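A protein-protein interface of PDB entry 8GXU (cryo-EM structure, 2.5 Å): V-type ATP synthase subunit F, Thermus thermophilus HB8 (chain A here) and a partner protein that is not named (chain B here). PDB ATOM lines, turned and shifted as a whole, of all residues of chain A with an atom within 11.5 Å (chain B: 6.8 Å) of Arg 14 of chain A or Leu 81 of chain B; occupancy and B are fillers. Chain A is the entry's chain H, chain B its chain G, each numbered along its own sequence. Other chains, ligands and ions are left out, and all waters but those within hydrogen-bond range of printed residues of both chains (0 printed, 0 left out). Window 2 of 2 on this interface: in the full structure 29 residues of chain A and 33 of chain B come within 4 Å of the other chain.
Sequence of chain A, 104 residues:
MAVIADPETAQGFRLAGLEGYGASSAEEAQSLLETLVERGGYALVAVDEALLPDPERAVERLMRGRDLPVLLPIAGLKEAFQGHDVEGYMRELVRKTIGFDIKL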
ATOM      1  N   MET A   1     -19.049  -3.714  14.324  1.00  0.00           N
ATOM      2  CA  MET A   1     -18.018  -2.778  14.854  1.00  0.00           C
ATOM      3  C   MET A   1     -18.651  -1.763  15.794  1.00  0.00           C
ATOM      4  O   MET A   1     -19.831  -1.863  16.126  1.00  0.00           O
ATOM      5  CB  MET A   1     -17.305  -2.054  13.709  1.00  0.00           C
ATOM      6  CG  MET A   1     -16.589  -2.981  12.746  1.00  0.00           C
ATOM      7  SD  MET A   1     -15.623  -2.086  11.515  1.00  0.00           S
ATOM      8  CE  MET A   1     -16.925  -1.329  10.548  1.00  0.00           C
ATOM      9  N   ALA A   2     -17.855  -0.788  16.224  1.00  0.00           N
ATOM     10  CA  ALA A   2     -18.334   0.264  17.108  1.00  0.00           C
ATOM     11  C   ALA A   2     -17.288   1.365  17.150  1.00  0.00           C
ATOM     12  O   ALA A   2     -16.180   1.216  16.629  1.00  0.00           O
ATOM     13  CB  ALA A   2     -18.626  -0.272  18.513  1.00  0.00           C
ATOM     14  N   VAL A   3     -17.656   2.480  17.777  1.00  0.00           N
ATOM     15  CA  VAL A   3     -16.750   3.608  17.951  1.00  0.00           C
ATOM     16  C   VAL A   3     -17.135   4.348  19.221  1.00  0.00           C
ATOM     17  O   VAL A   3     -18.307   4.401  19.603  1.00  0.00           O
ATOM     18  CB  VAL A   3     -16.776   4.563  16.733  1.00  0.00           C
ATOM     19  CG1 VAL A   3     -15.926   5.792  17.002  1.00  0.00           C
ATOM     20  CG2 VAL A   3     -16.297   3.850  15.481  1.00  0.00           C
ATOM     21  N   ILE A   4     -16.132   4.921  19.879  1.00  0.00           N
ATOM     22  CA  ILE A   4     -16.321   5.828  21.001  1.00  0.00           C
ATOM     23  C   ILE A   4     -15.650   7.147  20.652  1.00  0.00           C
ATOM     24  O   ILE A   4     -14.481   7.167  20.249  1.00  0.00           O
ATOM     25  CB  ILE A   4     -15.745   5.254  22.307  1.00  0.00           C
ATOM     26  CG1 ILE A   4     -16.479   3.963  22.686  1.00  0.00           C
ATOM     27  CG2 ILE A   4     -15.832   6.285  23.422  1.00  0.00           C
ATOM     28  CD1 ILE A   4     -15.788   3.152  23.764  1.00  0.00           C
ATOM     29  N   ALA A   5     -16.386   8.241  20.800  1.00  0.00           N
ATOM     30  CA  ALA A   5     -15.857   9.570  20.531  1.00  0.00           C
ATOM     31  C   ALA A   5     -16.782  10.589  21.188  1.00  0.00           C
ATOM     32  O   ALA A   5     -17.677  10.235  21.961  1.00  0.00           O
ATOM     33  CB  ALA A   5     -15.714   9.802  19.024  1.00  0.00           C
ATOM     34  N   ASP A   6     -16.565  11.863  20.879  1.00  0.00           N
ATOM     35  CA  ASP A   6     -17.446  12.898  21.386  1.00  0.00           C
ATOM     36  C   ASP A   6     -18.854  12.678  20.837  1.00  0.00           C
ATOM     37  O   ASP A   6     -19.022  12.172  19.723  1.00  0.00           O
ATOM     38  CB  ASP A   6     -16.937  14.280  20.984  1.00  0.00           C
ATOM     39  CG  ASP A   6     -15.587  14.602  21.591  1.00  0.00           C
ATOM     40  OD1 ASP A   6     -15.431  14.441  22.819  1.00  0.00           O
ATOM     41  OD2 ASP A   6     -14.680  15.018  20.839  1.00  0.00           O
ATOM     42  N   PRO A   7     -19.889  13.049  21.594  1.00  0.00           N
ATOM     43  CA  PRO A   7     -21.256  12.839  21.092  1.00  0.00           C
ATOM     44  C   PRO A   7     -21.522  13.542  19.775  1.00  0.00           C
ATOM     45  O   PRO A   7     -22.398  13.107  19.017  1.00  0.00           O
ATOM     46  CB  PRO A   7     -22.136  13.397  22.218  1.00  0.00           C
ATOM     47  CG  PRO A   7     -21.273  13.399  23.428  1.00  0.00           C
ATOM     48  CD  PRO A   7     -19.879  13.627  22.947  1.00  0.00           C
ATOM     49  N   GLU A   8     -20.791  14.617  19.477  1.00  0.00           N
ATOM     50  CA  GLU A   8     -21.026  15.351  18.240  1.00  0.00           C
ATOM     51  C   GLU A   8     -20.750  14.492  17.014  1.00  0.00           C
ATOM     52  O   GLU A   8     -21.450  14.612  16.003  1.00  0.00           O
ATOM     53  CB  GLU A   8     -20.160  16.610  18.205  1.00  0.00           C
ATOM     54  CG  GLU A   8     -20.457  17.598  19.322  1.00  0.00           C
ATOM     55  CD  GLU A   8     -19.732  18.916  19.141  1.00  0.00           C
ATOM     56  OE1 GLU A   8     -18.497  18.896  18.957  1.00  0.00           O
ATOM     57  OE2 GLU A   8     -20.397  19.973  19.183  1.00  0.00           O
ATOM     58  N   THR A   9     -19.733  13.635  17.074  1.00  0.00           N
ATOM     59  CA  THR A   9     -19.399  12.758  15.960  1.00  0.00           C
ATOM     60  C   THR A   9     -20.051  11.390  16.062  1.00  0.00           C
ATOM     61  O   THR A   9     -20.250  10.733  15.034  1.00  0.00           O
ATOM     62  CB  THR A   9     -17.879  12.584  15.860  1.00  0.00           C
ATOM     63  OG1 THR A   9     -17.552  11.875  14.658  1.00  0.00           O
ATOM     64  CG2 THR A   9     -17.333  11.826  17.069  1.00  0.00           C
ATOM     65  N   ALA A  10     -20.380  10.940  17.274  1.00  0.00           N
ATOM     66  CA  ALA A  10     -21.020   9.639  17.417  1.00  0.00           C
ATOM     67  C   ALA A  10     -22.330   9.585  16.649  1.00  0.00           C
ATOM     68  O   ALA A  10     -22.684   8.539  16.094  1.00  0.00           O
ATOM     69  CB  ALA A  10     -21.255   9.331  18.896  1.00  0.00           C
ATOM     70  N   GLN A  11     -23.062  10.697  16.605  1.00  0.00           N
ATOM     71  CA  GLN A  11     -24.308  10.712  15.852  1.00  0.00           C
ATOM     72  C   GLN A  11     -24.052  10.426  14.381  1.00  0.00           C
ATOM     73  O   GLN A  11     -24.770   9.635  13.763  1.00  0.00           O
ATOM     74  CB  GLN A  11     -25.014  12.058  16.028  1.00  0.00           C
ATOM     75  CG  GLN A  11     -24.201  13.255  15.573  1.00  0.00           C
ATOM     76  CD  GLN A  11     -24.854  14.575  15.933  1.00  0.00           C
ATOM     77  OE1 GLN A  11     -26.036  14.622  16.271  1.00  0.00           O
ATOM     78  NE2 GLN A  11     -24.083  15.654  15.863  1.00  0.00           N
ATOM     79  N   GLY A  12     -23.016  11.037  13.806  1.00  0.00           N
ATOM     80  CA  GLY A  12     -22.686  10.752  12.418  1.00  0.00           C
ATOM     81  C   GLY A  12     -22.206   9.328  12.214  1.00  0.00           C
ATOM     82  O   GLY A  12     -22.566   8.674  11.229  1.00  0.00           O
ATOM     83  N   PHE A  13     -21.378   8.829  13.135  1.00  0.00           N
ATOM     84  CA  PHE A  13     -20.928   7.444  13.040  1.00  0.00           C
ATOM     85  C   PHE A  13     -22.115   6.494  13.006  1.00  0.00           C
ATOM     86  O   PHE A  13     -22.144   5.548  12.210  1.00  0.00           O
ATOM     87  CB  PHE A  13     -20.007   7.104  14.213  1.00  0.00           C
ATOM     88  CG  PHE A  13     -18.606   7.629  14.063  1.00  0.00           C
ATOM     89  CD1 PHE A  13     -17.850   7.320  12.943  1.00  0.00           C
ATOM     90  CD2 PHE A  13     -18.041   8.421  15.048  1.00  0.00           C
ATOM     91  CE1 PHE A  13     -16.561   7.798  12.806  1.00  0.00           C
ATOM     92  CE2 PHE A  13     -16.751   8.901  14.915  1.00  0.00           C
ATOM     93  CZ  PHE A  13     -16.011   8.589  13.793  1.00  0.00           C
ATOM     94  N   ARG A  14     -23.109   6.730  13.864  1.00  0.00           N
ATOM     95  CA  ARG A  14     -24.319   5.920  13.822  1.00  0.00           C
ATOM     96  C   ARG A  14     -25.092   6.163  12.538  1.00  0.00           C
ATOM     97  O   ARG A  14     -25.702   5.236  11.994  1.00  0.00           O
ATOM     98  CB  ARG A  14     -25.191   6.215  15.041  1.00  0.00           C
ATOM     99  CG  ARG A  14     -26.335   5.237  15.227  1.00  0.00           C
ATOM    100  CD  ARG A  14     -27.069   5.480  16.536  1.00  0.00           C
ATOM    101  NE  ARG A  14     -28.218   4.598  16.695  1.00  0.00           N
ATOM    102  CZ  ARG A  14     -28.892   4.438  17.827  1.00  0.00           C
ATOM    103  NH1 ARG A  14     -28.555   5.086  18.929  1.00  0.00           N
ATOM    104  NH2 ARG A  14     -29.928   3.606  17.853  1.00  0.00           N
ATOM    105  N   LEU A  15     -25.066   7.394  12.034  1.00  0.00           N
ATOM    106  CA  LEU A  15     -25.697   7.682  10.754  1.00  0.00           C
ATOM    107  C   LEU A  15     -25.087   6.844   9.638  1.00  0.00           C
ATOM    108  O   LEU A  15     -25.756   6.558   8.640  1.00  0.00           O
ATOM    109  CB  LEU A  15     -25.569   9.174  10.445  1.00  0.00           C
ATOM    110  CG  LEU A  15     -26.225   9.669   9.158  1.00  0.00           C
ATOM    111  CD1 LEU A  15     -27.696   9.283   9.111  1.00  0.00           C
ATOM    112  CD2 LEU A  15     -26.061  11.175   9.029  1.00  0.00           C
ATOM    113  N   ALA A  16     -23.828   6.442   9.787  1.00  0.00           N
ATOM    114  CA  ALA A  16     -23.190   5.546   8.830  1.00  0.00           C
ATOM    115  C   ALA A  16     -23.362   4.071   9.176  1.00  0.00           C
ATOM    116  O   ALA A  16     -22.924   3.218   8.398  1.00  0.00           O
ATOM    117  CB  ALA A  16     -21.698   5.864   8.716  1.00  0.00           C
ATOM    118  N   GLY A  17     -23.983   3.748  10.309  1.00  0.00           N
ATOM    119  CA  GLY A  17     -24.226   2.371  10.684  1.00  0.00           C
ATOM    120  C   GLY A  17     -23.297   1.809  11.738  1.00  0.00           C
ATOM    121  O   GLY A  17     -23.392   0.615  12.045  1.00  0.00           O
ATOM    122  N   LEU A  18     -22.407   2.620  12.299  1.00  0.00           N
ATOM    123  CA  LEU A  18     -21.525   2.172  13.367  1.00  0.00           C
ATOM    124  C   LEU A  18     -22.172   2.438  14.718  1.00  0.00           C
ATOM    125  O   LEU A  18     -22.816   3.468  14.920  1.00  0.00           O
ATOM    126  CB  LEU A  18     -20.174   2.885  13.286  1.00  0.00           C
ATOM    127  CG  LEU A  18     -19.421   2.735  11.962  1.00  0.00           C
ATOM    128  CD1 LEU A  18     -18.135   3.546  11.984  1.00  0.00           C
ATOM    129  CD2 LEU A  18     -19.130   1.273  11.666  1.00  0.00           C
ATOM    130  N   GLU A  19     -21.990   1.503  15.649  1.00  0.00           N
ATOM    131  CA  GLU A  19     -22.577   1.626  16.981  1.00  0.00           C
ATOM    132  C   GLU A  19     -21.793   2.692  17.739  1.00  0.00           C
ATOM    133  O   GLU A  19     -20.914   2.411  18.557  1.00  0.00           O
ATOM    134  CB  GLU A  19     -22.552   0.286  17.708  1.00  0.00           C
ATOM    135  CG  GLU A  19     -23.338   0.265  19.009  1.00  0.00           C
ATOM    136  CD  GLU A  19     -24.830   0.098  18.789  1.00  0.00           C
ATOM    137  OE1 GLU A  19     -25.424   0.930  18.073  1.00  0.00           O
ATOM    138  OE2 GLU A  19     -25.407  -0.865  19.335  1.00  0.00           O
ATOM    139  N   GLY A  20     -22.118   3.948  17.451  1.00  0.00           N
ATOM    140  CA  GLY A  20     -21.403   5.049  18.051  1.00  0.00           C
ATOM    141  C   GLY A  20     -21.791   5.284  19.497  1.00  0.00           C
ATOM    142  O   GLY A  20     -22.842   4.860  19.971  1.00  0.00           O
ATOM    143  N   TYR A  21     -20.906   5.977  20.207  1.00  0.00           N
ATOM    144  CA  TYR A  21     -21.137   6.338  21.596  1.00  0.00           C
ATOM    145  C   TYR A  21     -20.513   7.696  21.872  1.00  0.00           C
ATOM    146  O   TYR A  21     -19.570   8.114  21.196  1.00  0.00           O
ATOM    147  CB  TYR A  21     -20.560   5.295  22.555  1.00  0.00           C
ATOM    148  CG  TYR A  21     -21.211   3.937  22.435  1.00  0.00           C
ATOM    149  CD1 TYR A  21     -20.801   3.030  21.472  1.00  0.00           C
ATOM    150  CD2 TYR A  21     -22.234   3.560  23.293  1.00  0.00           C
ATOM    151  CE1 TYR A  21     -21.392   1.790  21.361  1.00  0.00           C
ATOM    152  CE2 TYR A  21     -22.833   2.321  23.192  1.00  0.00           C
ATOM    153  CZ  TYR A  21     -22.407   1.439  22.223  1.00  0.00           C
ATOM    154  OH  TYR A  21     -23.000   0.202  22.117  1.00  0.00           O
ATOM    155  N   GLY A  22     -21.051   8.380  22.879  1.00  0.00           N
ATOM    156  CA  GLY A  22     -20.562   9.687  23.274  1.00  0.00           C
ATOM    157  C   GLY A  22     -19.699   9.579  24.518  1.00  0.00           C
ATOM    158  O   GLY A  22     -20.116   9.011  25.530  1.00  0.00           O
ATOM    159  N   TYR A  42     -18.680  -6.918  18.972  1.00  0.00           N
ATOM    160  CA  TYR A  42     -18.096  -6.213  17.837  1.00  0.00           C
ATOM    161  C   TYR A  42     -16.578  -6.345  17.827  1.00  0.00           C
ATOM    162  O   TYR A  42     -15.941  -6.545  18.864  1.00  0.00           O
ATOM    163  CB  TYR A  42     -18.501  -4.740  17.886  1.00  0.00           C
ATOM    164  CG  TYR A  42     -19.982  -4.535  18.112  1.00  0.00           C
ATOM    165  CD1 TYR A  42     -20.913  -5.424  17.590  1.00  0.00           C
ATOM    166  CD2 TYR A  42     -20.447  -3.465  18.859  1.00  0.00           C
ATOM    167  CE1 TYR A  42     -22.265  -5.247  17.798  1.00  0.00           C
ATOM    168  CE2 TYR A  42     -21.800  -3.277  19.073  1.00  0.00           C
ATOM    169  CZ  TYR A  42     -22.704  -4.172  18.539  1.00  0.00           C
ATOM    170  OH  TYR A  42     -24.052  -3.991  18.748  1.00  0.00           O
ATOM    171  N   ALA A  46     -12.672   2.017  17.371  1.00  0.00           N
ATOM    172  CA  ALA A  46     -11.831   3.198  17.261  1.00  0.00           C
ATOM    173  C   ALA A  46     -12.140   4.158  18.401  1.00  0.00           C
ATOM    174  O   ALA A  46     -13.304   4.440  18.693  1.00  0.00           O
ATOM    175  CB  ALA A  46     -12.045   3.894  15.918  1.00  0.00           C
ATOM    176  N   ILE A  74      -8.249   7.316  16.735  1.00  0.00           N
ATOM    177  CA  ILE A  74      -8.868   8.086  15.667  1.00  0.00           C
ATOM    178  C   ILE A  74      -8.766   9.563  16.011  1.00  0.00           C
ATOM    179  O   ILE A  74      -8.772   9.952  17.184  1.00  0.00           O
ATOM    180  CB  ILE A  74     -10.335   7.661  15.448  1.00  0.00           C
ATOM    181  CG1 ILE A  74     -10.845   8.182  14.105  1.00  0.00           C
ATOM    182  CG2 ILE A  74     -11.206   8.150  16.587  1.00  0.00           C
ATOM    183  CD1 ILE A  74     -12.167   7.577  13.683  1.00  0.00           C
ATOM    184  N   LEU A  77     -12.177  15.881  16.450  1.00  0.00           N
ATOM    185  CA  LEU A  77     -12.964  16.665  15.504  1.00  0.00           C
ATOM    186  C   LEU A  77     -12.402  18.073  15.342  1.00  0.00           C
ATOM    187  O   LEU A  77     -11.942  18.446  14.258  1.00  0.00           O
ATOM    188  CB  LEU A  77     -14.423  16.717  15.963  1.00  0.00           C
ATOM    189  CG  LEU A  77     -15.267  15.459  15.739  1.00  0.00           C
ATOM    190  CD1 LEU A  77     -15.126  14.926  14.323  1.00  0.00           C
ATOM    191  CD2 LEU A  77     -14.889  14.390  16.747  1.00  0.00           C
ATOM    192  N   GLU B  74     -32.545  17.574  15.524  1.00  0.00           N
ATOM    193  CA  GLU B  74     -33.440  16.475  15.864  1.00  0.00           C
ATOM    194  C   GLU B  74     -33.606  15.531  14.682  1.00  0.00           C
ATOM    195  O   GLU B  74     -33.696  14.313  14.860  1.00  0.00           O
ATOM    196  CB  GLU B  74     -34.795  17.018  16.314  1.00  0.00           C
ATOM    197  CG  GLU B  74     -34.731  17.928  17.533  1.00  0.00           C
ATOM    198  CD  GLU B  74     -34.567  19.391  17.168  1.00  0.00           C
ATOM    199  OE1 GLU B  74     -34.165  19.679  16.021  1.00  0.00           O
ATOM    200  OE2 GLU B  74     -34.841  20.254  18.028  1.00  0.00           O
ATOM    201  N   VAL B  76     -31.362  14.880  12.349  1.00  0.00           N
ATOM    202  CA  VAL B  76     -30.146  14.076  12.264  1.00  0.00           C
ATOM    203  C   VAL B  76     -30.128  13.025  13.364  1.00  0.00           C
ATOM    204  O   VAL B  76     -29.746  11.870  13.135  1.00  0.00           O
ATOM    205  CB  VAL B  76     -28.903  14.984  12.327  1.00  0.00           C
ATOM    206  CG1 VAL B  76     -27.640  14.149  12.482  1.00  0.00           C
ATOM    207  CG2 VAL B  76     -28.822  15.862  11.087  1.00  0.00           C
ATOM    208  N   ALA B  77     -30.520  13.408  14.581  1.00  0.00           N
ATOM    209  CA  ALA B  77     -30.548  12.447  15.678  1.00  0.00           C
ATOM    210  C   ALA B  77     -31.513  11.307  15.379  1.00  0.00           C
ATOM    211  O   ALA B  77     -31.202  10.137  15.630  1.00  0.00           O
ATOM    212  CB  ALA B  77     -30.930  13.149  16.981  1.00  0.00           C
ATOM    213  N   GLY B  78     -32.690  11.631  14.844  1.00  0.00           N
ATOM    214  CA  GLY B  78     -33.639  10.590  14.490  1.00  0.00           C
ATOM    215  C   GLY B  78     -33.120   9.689  13.389  1.00  0.00           C
ATOM    216  O   GLY B  78     -33.319   8.473  13.423  1.00  0.00           O
ATOM    217  N   ALA B  79     -32.449  10.273  12.395  1.00  0.00           N
ATOM    218  CA  ALA B  79     -31.875   9.462  11.328  1.00  0.00           C
ATOM    219  C   ALA B  79     -30.827   8.507  11.880  1.00  0.00           C
ATOM    220  O   ALA B  79     -30.779   7.332  11.495  1.00  0.00           O
ATOM    221  CB  ALA B  79     -31.267  10.363  10.252  1.00  0.00           C
ATOM    222  N   ALA B  80     -29.979   8.993  12.789  1.00  0.00           N
ATOM    223  CA  ALA B  80     -28.988   8.124  13.412  1.00  0.00           C
ATOM    224  C   ALA B  80     -29.657   7.017  14.215  1.00  0.00           C
ATOM    225  O   ALA B  80     -29.242   5.854  14.152  1.00  0.00           O
ATOM    226  CB  ALA B  80     -28.058   8.946  14.303  1.00  0.00           C
ATOM    227  N   LEU B  81     -30.703   7.358  14.972  1.00  0.00           N
ATOM    228  CA  LEU B  81     -31.393   6.351  15.771  1.00  0.00           C
ATOM    229  C   LEU B  81     -32.013   5.276  14.887  1.00  0.00           C
ATOM    230  O   LEU B  81     -31.952   4.084  15.210  1.00  0.00           O
ATOM    231  CB  LEU B  81     -32.465   7.014  16.637  1.00  0.00           C
ATOM    232  CG  LEU B  81     -31.945   7.833  17.820  1.00  0.00           C
ATOM    233  CD1 LEU B  81     -32.978   8.860  18.254  1.00  0.00           C
ATOM    234  CD2 LEU B  81     -31.571   6.922  18.979  1.00  0.00           C
ATOM    235  N   GLY B  82     -32.614   5.679  13.767  1.00  0.00           N
ATOM    236  CA  GLY B  82     -33.229   4.704  12.881  1.00  0.00           C
ATOM    237  C   GLY B  82     -32.225   3.726  12.299  1.00  0.00           C
ATOM    238  O   GLY B  82     -32.492   2.525  12.212  1.00  0.00           O
ATOM    239  N   VAL B  83     -31.059   4.223  11.896  1.00  0.00           N
ATOM    240  CA  VAL B  83     -30.054   3.344  11.289  1.00  0.00           C
ATOM    241  C   VAL B  83     -29.577   2.334  12.327  1.00  0.00           C
ATOM    242  O   VAL B  83     -29.140   2.735  13.424  1.00  0.00           O
ATOM    243  CB  VAL B  83     -28.875   4.170  10.745  1.00  0.00           C
ATOM    244  CG1 VAL B  83     -27.739   3.257  10.310  1.00  0.00           C
ATOM    245  CG2 VAL B  83     -29.330   5.049   9.590  1.00  0.00           C
ATOM    246  N   PRO B  84     -29.632   1.032  12.054  1.00  0.00           N
ATOM    247  CA  PRO B  84     -29.201   0.049  13.048  1.00  0.00           C
ATOM    248  C   PRO B  84     -27.706  -0.201  12.963  1.00  0.00           C
ATOM    249  O   PRO B  84     -27.069   0.127  11.950  1.00  0.00           O
ATOM    250  CB  PRO B  84     -29.998  -1.203  12.663  1.00  0.00           C
ATOM    251  CG  PRO B  84     -30.119  -1.098  11.178  1.00  0.00           C
ATOM    252  CD  PRO B  84     -30.168   0.380  10.844  1.00  0.00           C
ATOM    253  N   PRO B  85     -27.106  -0.786  14.005  1.00  0.00           N
ATOM    254  CA  PRO B  85     -25.687  -1.155  13.923  1.00  0.00           C
ATOM    255  C   PRO B  85     -25.483  -2.385  13.054  1.00  0.00           C
ATOM    256  O   PRO B  85     -25.312  -3.498  13.560  1.00  0.00           O
ATOM    257  CB  PRO B  85     -25.307  -1.416  15.385  1.00  0.00           C
ATOM    258  CG  PRO B  85     -26.582  -1.834  16.035  1.00  0.00           C
ATOM    259  CD  PRO B  85     -27.693  -1.115  15.317  1.00  0.00           C
ATOM    260  N   LEU B 113     -29.167   0.121   6.276  1.00  0.00           N
ATOM    261  CA  LEU B 113     -29.352   1.418   6.917  1.00  0.00           C
ATOM    262  C   LEU B 113     -30.819   1.814   6.799  1.00  0.00           C
ATOM    263  O   LEU B 113     -31.310   2.083   5.697  1.00  0.00           O
ATOM    264  CB  LEU B 113     -28.445   2.464   6.276  1.00  0.00           C
ATOM    265  CG  LEU B 113     -26.958   2.351   6.617  1.00  0.00           C
ATOM    266  CD1 LEU B 113     -26.227   1.536   5.560  1.00  0.00           C
ATOM    267  CD2 LEU B 113     -26.331   3.729   6.763  1.00  0.00           C
ATOM    268  N   LEU B 114     -31.519   1.852   7.929  1.00  0.00           N
ATOM    269  CA  LEU B 114     -32.949   2.129   7.943  1.00  0.00           C
ATOM    270  C   LEU B 114     -33.198   3.602   8.242  1.00  0.00           C
ATOM    271  O   LEU B 114     -32.699   4.138   9.237  1.00  0.00           O
ATOM    272  CB  LEU B 114     -33.658   1.255   8.979  1.00  0.00           C
ATOM    273  CG  LEU B 114     -34.130  -0.122   8.500  1.00  0.00           C
ATOM    274  CD1 LEU B 114     -35.180   0.006   7.405  1.00  0.00           C
ATOM    275  CD2 LEU B 114     -32.952  -0.957   8.020  1.00  0.00           C
ATOM    276  N   SER B 127     -24.489  10.716   5.630  1.00  0.00           N
ATOM    277  CA  SER B 127     -24.313   9.289   5.861  1.00  0.00           C
ATOM    278  C   SER B 127     -23.316   8.699   4.873  1.00  0.00           C
ATOM    279  O   SER B 127     -22.523   7.823   5.232  1.00  0.00           O
ATOM    280  CB  SER B 127     -25.657   8.570   5.766  1.00  0.00           C
ATOM    281  OG  SER B 127     -25.532   7.214   6.159  1.00  0.00           O
ATOM    282  N   PHE B 130     -19.797   9.545   6.013  1.00  0.00           N
ATOM    283  CA  PHE B 130     -19.363   8.777   7.170  1.00  0.00           C
ATOM    284  C   PHE B 130     -19.175   7.303   6.833  1.00  0.00           C
ATOM    285  O   PHE B 130     -18.330   6.638   7.439  1.00  0.00           O
ATOM    286  CB  PHE B 130     -20.352   8.964   8.314  1.00  0.00           C
ATOM    287  CG  PHE B 130     -19.991  10.083   9.230  1.00  0.00           C
ATOM    288  CD1 PHE B 130     -19.972  11.384   8.774  1.00  0.00           C
ATOM    289  CD2 PHE B 130     -19.676   9.835  10.550  1.00  0.00           C
ATOM    290  CE1 PHE B 130     -19.637  12.419   9.616  1.00  0.00           C
ATOM    291  CE2 PHE B 130     -19.345  10.865  11.402  1.00  0.00           C
ATOM    292  CZ  PHE B 130     -19.325  12.160  10.934  1.00  0.00           C
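Printed residues of chain B that touch a printed residue of chain A: Ala 79, Ala 80, Leu 81, Val 83, Pro 84, Pro 85, Leu 113, Ser 127 and Phe 130. Hydrophobic or aromatic side chains of chain B that line the printed part of chain A: Ala 79, Ala 80, Leu 81, Val 83, Pro 85, Leu 113 and Phe 130. Among the printed residues, no Asp or Glu carboxylate lies within 4 Å of a Lys or Arg side-chain nitrogen of the other chain.
Of chain A, only Arg 14 (3.4 Å) comes within 4 Å of Leu 81 of chain B. No residue of chain A comes within 4 Å of Gly 82 of chain B. Of chain A, only Gly 17 (3.7 Å) comes within 4 Å of Pro 84 of chain B. Printed residues of chain B within 4 Å of Gly 12 of chain A: Phe 130 (3.1 Å). Of the printed residues of chain B, Phe 13 of chain A touches Phe 130 (3.3 Å). Printed residues of chain A within 4 Å of Leu 113 of chain B: Leu 15 and Ala 16. Of the printed residues of chain B, Leu 15 of chain A touches Ala 79 (3.9 Å), Val 83 (3.99 Å), Leu 113 (3.4 Å) and Ser 127 (2.6 Å). Pro 7 of chain A touches none of the printed residues of chain B. The nearest printed residue of chain A that does not touch Val 83 of chain B is Ala 16 of chain A (4.6 Å).
N of Val 83 of chain B is in hydrogen-bond range of O of Leu 114 of chain B, at 3.1 Å. The backbone carbonyl oxygen (O) of Glu 19 of chain A is in hydrogen-bond range of the backbone NH (N) of Val 3 of chain A (3.4 Å). The backbone carbonyl oxygen (O) of Glu 8 of chain A sits at hydrogen-bond distance from the side-chain amide nitrogen (NE2) of Gln 11 of chain A, at 2.8 Å. N of Leu 18 of chain A is in hydrogen-bond range of O of Phe 13 of chain A, 2.9 Å away. The side-chain hydroxyl (OH) of Tyr 42 of chain A sits at hydrogen-bond distance from the side-chain carboxylate (OE2) of Glu 19 of chain A.
Gln 11 of chain A touches Ala 80 of chain B (O to CB, 3.4 Å). Gly 12 of chain A touches Phe 130 of chain B. Leu 15 of chain A touches Val 83 of chain B (O to CG2, 3.99 Å). Leu 15 of chain A touches Leu 113 of chain B. Leu 113 of chain B touches Ala 16 of chain A (CD2 to O, 3.8 Å). Ser 127 of chain B touches Ala 16 of chain A (OG to CA, 3.9 Å). Ala 16 of chain A touches Phe 130 of chain B. Val 83 of chain B touches Gly 17 of chain A. Gly 17 of chain A touches Pro 84 of chain B. Pro 85 of chain B touches Gly 17 of chain A (CA to O, 3.5 Å).
The guanidinium group (NE) of Arg 14 of chain A sits at hydrogen-bond distance from the backbone carbonyl oxygen (O) of Ala 80 of chain B, 3.0 Å away. The backbone carbonyl oxygen of Leu 81 of chain B is in hydrogen-bond range of the guanidinium group of Arg 14 of chain A. OG of Ser 127 of chain B is in hydrogen-bond range of O of Leu 15 of chain A, at 2.6 Å.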
